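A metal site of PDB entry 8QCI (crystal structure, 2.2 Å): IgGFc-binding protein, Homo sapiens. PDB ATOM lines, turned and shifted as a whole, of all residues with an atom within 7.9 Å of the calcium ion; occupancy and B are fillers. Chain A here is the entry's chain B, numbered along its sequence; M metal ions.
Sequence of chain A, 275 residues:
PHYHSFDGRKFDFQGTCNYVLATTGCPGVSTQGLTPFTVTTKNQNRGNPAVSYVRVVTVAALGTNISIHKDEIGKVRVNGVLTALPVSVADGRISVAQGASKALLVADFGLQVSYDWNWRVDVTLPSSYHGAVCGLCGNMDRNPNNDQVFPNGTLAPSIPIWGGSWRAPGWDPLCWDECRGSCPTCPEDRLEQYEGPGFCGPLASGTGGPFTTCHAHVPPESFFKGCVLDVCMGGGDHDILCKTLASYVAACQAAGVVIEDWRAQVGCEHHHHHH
The side-chain carboxylate of Asp 7 sits close to the backbone NH of Met 140. The backbone NH of Arg 142 lies within hydrogen-bond range of the side-chain carboxylate of Asp 7, 2.8 Å away. N of Asp 7 lies close to OG of Ser 5 (3.3 Å). O of Asn 139 is in hydrogen-bond range of N of Gly 131. OD1 of Asn 143 is in hydrogen-bond range of N of Asn 145, 3.1 Å away. OG of Ser 5 sits at hydrogen-bond distance from OD2 of Asp 147 (3.1 Å).
Of the 19 residues printed, 6 come within 4 Å of the calcium ion.
The calcium ion is bound by OD2 of Asp 7 (2.2 Å), OD1 of Asn 139 (2.3 Å), O of Asn 143 (2.3 Å), OD1 of Asp 147 (2.4 Å), OD1 of Asn 146 (2.4 Å) and OD1 of Asp 141 (2.5 Å). The calcium ion has six donor atoms within binding distance.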
ATOM      1  N   SER A   5     -21.663  15.226  16.719  1.00  0.00           N
ATOM      2  CA  SER A   5     -22.961  14.636  17.015  1.00  0.00           C
ATOM      3  C   SER A   5     -23.954  14.906  15.886  1.00  0.00           C
ATOM      4  O   SER A   5     -23.707  15.738  15.001  1.00  0.00           O
ATOM      5  CB  SER A   5     -23.496  15.172  18.345  1.00  0.00           C
ATOM      6  OG  SER A   5     -24.102  16.435  18.138  1.00  0.00           O
ATOM      7  N   PHE A   6     -25.090  14.212  15.925  1.00  0.00           N
ATOM      8  CA  PHE A   6     -26.142  14.466  14.928  1.00  0.00           C
ATOM      9  C   PHE A   6     -26.464  15.954  14.847  1.00  0.00           C
ATOM     10  O   PHE A   6     -26.565  16.515  13.743  1.00  0.00           O
ATOM     11  CB  PHE A   6     -27.414  13.699  15.245  1.00  0.00           C
ATOM     12  CG  PHE A   6     -27.366  12.255  14.863  1.00  0.00           C
ATOM     13  CD1 PHE A   6     -27.165  11.888  13.537  1.00  0.00           C
ATOM     14  CD2 PHE A   6     -27.539  11.271  15.819  1.00  0.00           C
ATOM     15  CE1 PHE A   6     -27.127  10.572  13.187  1.00  0.00           C
ATOM     16  CE2 PHE A   6     -27.500   9.945  15.470  1.00  0.00           C
ATOM     17  CZ  PHE A   6     -27.293   9.591  14.155  1.00  0.00           C
ATOM     18  N   ASP A   7     -26.609  16.594  15.993  1.00  0.00           N
ATOM     19  CA  ASP A   7     -26.933  18.014  16.109  1.00  0.00           C
ATOM     20  C   ASP A   7     -25.728  18.924  15.963  1.00  0.00           C
ATOM     21  O   ASP A   7     -25.860  20.129  16.221  1.00  0.00           O
ATOM     22  CB  ASP A   7     -27.619  18.275  17.447  1.00  0.00           C
ATOM     23  CG  ASP A   7     -28.958  17.602  17.536  1.00  0.00           C
ATOM     24  OD1 ASP A   7     -29.549  17.355  16.467  1.00  0.00           O
ATOM     25  OD2 ASP A   7     -29.392  17.285  18.645  1.00  0.00           O
ATOM     26  N   GLY A   8     -24.566  18.406  15.587  1.00  0.00           N
ATOM     27  CA  GLY A   8     -23.434  19.246  15.276  1.00  0.00           C
ATOM     28  C   GLY A   8     -22.537  19.645  16.434  1.00  0.00           C
ATOM     29  O   GLY A   8     -21.741  20.579  16.283  1.00  0.00           O
ATOM     30  N   ARG A   9     -22.634  18.980  17.575  1.00  0.00           N
ATOM     31  CA  ARG A   9     -21.697  19.257  18.656  1.00  0.00           C
ATOM     32  C   ARG A   9     -20.371  18.537  18.402  1.00  0.00           C
ATOM     33  O   ARG A   9     -20.336  17.310  18.216  1.00  0.00           O
ATOM     34  CB  ARG A   9     -22.284  18.846  19.999  1.00  0.00           C
ATOM     35  CG  ARG A   9     -21.290  18.931  21.163  1.00  0.00           C
ATOM     36  CD  ARG A   9     -22.004  18.587  22.463  1.00  0.00           C
ATOM     37  NE  ARG A   9     -21.285  17.697  23.368  1.00  0.00           N
ATOM     38  CZ  ARG A   9     -21.502  16.394  23.470  1.00  0.00           C
ATOM     39  NH1 ARG A   9     -22.282  15.758  22.615  1.00  0.00           N
ATOM     40  NH2 ARG A   9     -20.928  15.725  24.463  1.00  0.00           N
ATOM     41  N   GLY A 131     -35.146  13.419  17.513  1.00  0.00           N
ATOM     42  CA  GLY A 131     -35.528  13.269  18.894  1.00  0.00           C
ATOM     43  C   GLY A 131     -35.804  11.852  19.331  1.00  0.00           C
ATOM     44  O   GLY A 131     -36.222  11.644  20.470  1.00  0.00           O
ATOM     45  N   VAL A 133     -33.539   9.089  19.134  1.00  0.00           N
ATOM     46  CA  VAL A 133     -32.335   8.286  19.329  1.00  0.00           C
ATOM     47  C   VAL A 133     -31.535   8.876  20.488  1.00  0.00           C
ATOM     48  O   VAL A 133     -31.806   9.987  20.963  1.00  0.00           O
ATOM     49  CB  VAL A 133     -31.453   8.230  18.066  1.00  0.00           C
ATOM     50  CG1 VAL A 133     -32.150   7.432  16.983  1.00  0.00           C
ATOM     51  CG2 VAL A 133     -31.180   9.641  17.598  1.00  0.00           C
ATOM     52  N   CYS A 137     -23.917  10.007  20.137  1.00  0.00           N
ATOM     53  CA  CYS A 137     -24.303  10.936  19.074  1.00  0.00           C
ATOM     54  C   CYS A 137     -25.407  11.908  19.476  1.00  0.00           C
ATOM     55  O   CYS A 137     -25.762  12.775  18.680  1.00  0.00           O
ATOM     56  CB  CYS A 137     -24.745  10.155  17.827  1.00  0.00           C
ATOM     57  SG  CYS A 137     -23.404   9.270  16.974  1.00  0.00           S
ATOM     58  N   GLY A 138     -25.989  11.788  20.665  1.00  0.00           N
ATOM     59  CA  GLY A 138     -27.071  12.685  21.031  1.00  0.00           C
ATOM     60  C   GLY A 138     -28.427  12.247  20.478  1.00  0.00           C
ATOM     61  O   GLY A 138     -28.601  11.097  20.018  1.00  0.00           O
ATOM     62  N   ASN A 139     -29.395  13.174  20.515  1.00  0.00           N
ATOM     63  CA  ASN A 139     -30.775  12.837  20.212  1.00  0.00           C
ATOM     64  C   ASN A 139     -31.289  13.417  18.893  1.00  0.00           C
ATOM     65  O   ASN A 139     -32.472  13.252  18.597  1.00  0.00           O
ATOM     66  CB  ASN A 139     -31.715  13.273  21.346  1.00  0.00           C
ATOM     67  CG  ASN A 139     -31.618  14.762  21.697  1.00  0.00           C
ATOM     68  OD1 ASN A 139     -31.023  15.571  20.990  1.00  0.00           O
ATOM     69  ND2 ASN A 139     -32.258  15.132  22.804  1.00  0.00           N
ATOM     70  N   MET A 140     -30.446  14.071  18.094  1.00  0.00           N
ATOM     71  CA  MET A 140     -30.848  14.587  16.793  1.00  0.00           C
ATOM     72  C   MET A 140     -32.168  15.372  16.882  1.00  0.00           C
ATOM     73  O   MET A 140     -33.199  14.980  16.335  1.00  0.00           O
ATOM     74  CB  MET A 140     -30.952  13.450  15.755  1.00  0.00           C
ATOM     75  CG  MET A 140     -31.149  13.924  14.283  1.00  0.00           C
ATOM     76  SD  MET A 140     -31.154  12.632  12.990  1.00  0.00           S
ATOM     77  CE  MET A 140     -32.452  11.635  13.592  1.00  0.00           C
ATOM     78  N   ASP A 141     -32.140  16.464  17.656  1.00  0.00           N
ATOM     79  CA  ASP A 141     -33.295  17.347  17.765  1.00  0.00           C
ATOM     80  C   ASP A 141     -32.946  18.771  17.368  1.00  0.00           C
ATOM     81  O   ASP A 141     -33.581  19.717  17.833  1.00  0.00           O
ATOM     82  CB  ASP A 141     -33.893  17.316  19.178  1.00  0.00           C
ATOM     83  CG  ASP A 141     -32.953  17.887  20.240  1.00  0.00           C
ATOM     84  OD1 ASP A 141     -31.901  18.465  19.892  1.00  0.00           O
ATOM     85  OD2 ASP A 141     -33.264  17.738  21.452  1.00  0.00           O
ATOM     86  N   ARG A 142     -31.921  18.921  16.530  1.00  0.00           N
ATOM     87  CA  ARG A 142     -31.422  20.207  16.044  1.00  0.00           C
ATOM     88  C   ARG A 142     -30.853  21.076  17.167  1.00  0.00           C
ATOM     89  O   ARG A 142     -30.495  22.232  16.934  1.00  0.00           O
ATOM     90  CB  ARG A 142     -32.513  20.965  15.270  1.00  0.00           C
ATOM     91  CG  ARG A 142     -32.692  20.529  13.792  1.00  0.00           C
ATOM     92  CD  ARG A 142     -33.441  19.186  13.616  1.00  0.00           C
ATOM     93  NE  ARG A 142     -32.891  18.384  12.515  1.00  0.00           N
ATOM     94  CZ  ARG A 142     -33.163  17.109  12.297  1.00  0.00           C
ATOM     95  NH1 ARG A 142     -34.002  16.428  13.058  1.00  0.00           N
ATOM     96  NH2 ARG A 142     -32.563  16.484  11.288  1.00  0.00           N
ATOM     97  N   ASN A 143     -30.763  20.543  18.390  1.00  0.00           N
ATOM     98  CA  ASN A 143     -30.179  21.290  19.502  1.00  0.00           C
ATOM     99  C   ASN A 143     -28.871  20.645  19.932  1.00  0.00           C
ATOM    100  O   ASN A 143     -28.887  19.573  20.556  1.00  0.00           O
ATOM    101  CB  ASN A 143     -31.137  21.362  20.682  1.00  0.00           C
ATOM    102  CG  ASN A 143     -30.593  22.170  21.827  1.00  0.00           C
ATOM    103  OD1 ASN A 143     -29.530  22.798  21.705  1.00  0.00           O
ATOM    104  ND2 ASN A 143     -31.284  22.158  22.952  1.00  0.00           N
ATOM    105  N   PRO A 144     -27.715  21.258  19.648  1.00  0.00           N
ATOM    106  CA  PRO A 144     -26.432  20.611  19.967  1.00  0.00           C
ATOM    107  C   PRO A 144     -26.094  20.627  21.440  1.00  0.00           C
ATOM    108  O   PRO A 144     -25.109  19.981  21.827  1.00  0.00           O
ATOM    109  CB  PRO A 144     -25.420  21.455  19.186  1.00  0.00           C
ATOM    110  CG  PRO A 144     -26.039  22.813  19.182  1.00  0.00           C
ATOM    111  CD  PRO A 144     -27.517  22.598  19.066  1.00  0.00           C
ATOM    112  N   ASN A 145     -26.860  21.320  22.260  1.00  0.00           N
ATOM    113  CA  ASN A 145     -26.440  21.675  23.613  1.00  0.00           C
ATOM    114  C   ASN A 145     -26.994  20.750  24.681  1.00  0.00           C
ATOM    115  O   ASN A 145     -26.558  20.825  25.827  1.00  0.00           O
ATOM    116  CB  ASN A 145     -26.851  23.123  23.900  1.00  0.00           C
ATOM    117  CG  ASN A 145     -25.980  24.110  23.167  1.00  0.00           C
ATOM    118  OD1 ASN A 145     -24.756  23.941  23.103  1.00  0.00           O
ATOM    119  ND2 ASN A 145     -26.597  25.104  22.546  1.00  0.00           N
ATOM    120  N   ASN A 146     -27.918  19.862  24.323  1.00  0.00           N
ATOM    121  CA  ASN A 146     -28.466  18.894  25.263  1.00  0.00           C
ATOM    122  C   ASN A 146     -28.056  17.468  24.920  1.00  0.00           C
ATOM    123  O   ASN A 146     -28.777  16.508  25.219  1.00  0.00           O
ATOM    124  CB  ASN A 146     -29.992  19.028  25.306  1.00  0.00           C
ATOM    125  CG  ASN A 146     -30.632  18.743  23.948  1.00  0.00           C
ATOM    126  OD1 ASN A 146     -29.940  18.644  22.943  1.00  0.00           O
ATOM    127  ND2 ASN A 146     -31.950  18.600  23.938  1.00  0.00           N
ATOM    128  N   ASP A 147     -26.885  17.295  24.290  1.00  0.00           N
ATOM    129  CA  ASP A 147     -26.478  16.001  23.772  1.00  0.00           C
ATOM    130  C   ASP A 147     -25.577  15.214  24.709  1.00  0.00           C
ATOM    131  O   ASP A 147     -25.299  14.045  24.422  1.00  0.00           O
ATOM    132  CB  ASP A 147     -25.756  16.176  22.434  1.00  0.00           C
ATOM    133  CG  ASP A 147     -26.709  16.513  21.306  1.00  0.00           C
ATOM    134  OD1 ASP A 147     -27.920  16.197  21.461  1.00  0.00           O
ATOM    135  OD2 ASP A 147     -26.255  17.064  20.284  1.00  0.00           O
ATOM    136  N   GLN A 148     -25.112  15.829  25.809  1.00  0.00           N
ATOM    137  CA  GLN A 148     -24.195  15.212  26.769  1.00  0.00           C
ATOM    138  C   GLN A 148     -25.013  14.894  28.007  1.00  0.00           C
ATOM    139  O   GLN A 148     -24.963  15.601  29.028  1.00  0.00           O
ATOM    140  CB  GLN A 148     -22.974  16.115  27.098  1.00  0.00           C
ATOM    141  CG  GLN A 148     -21.932  15.461  28.043  1.00  0.00           C
ATOM    142  CD  GLN A 148     -21.058  16.471  28.788  1.00  0.00           C
ATOM    143  OE1 GLN A 148     -20.995  16.470  30.024  1.00  0.00           O
ATOM    144  NE2 GLN A 148     -20.380  17.345  28.031  1.00  0.00           N
HETATM  145 CA    CA M   1     -29.830  17.501  20.826  1.00  0.00          CA
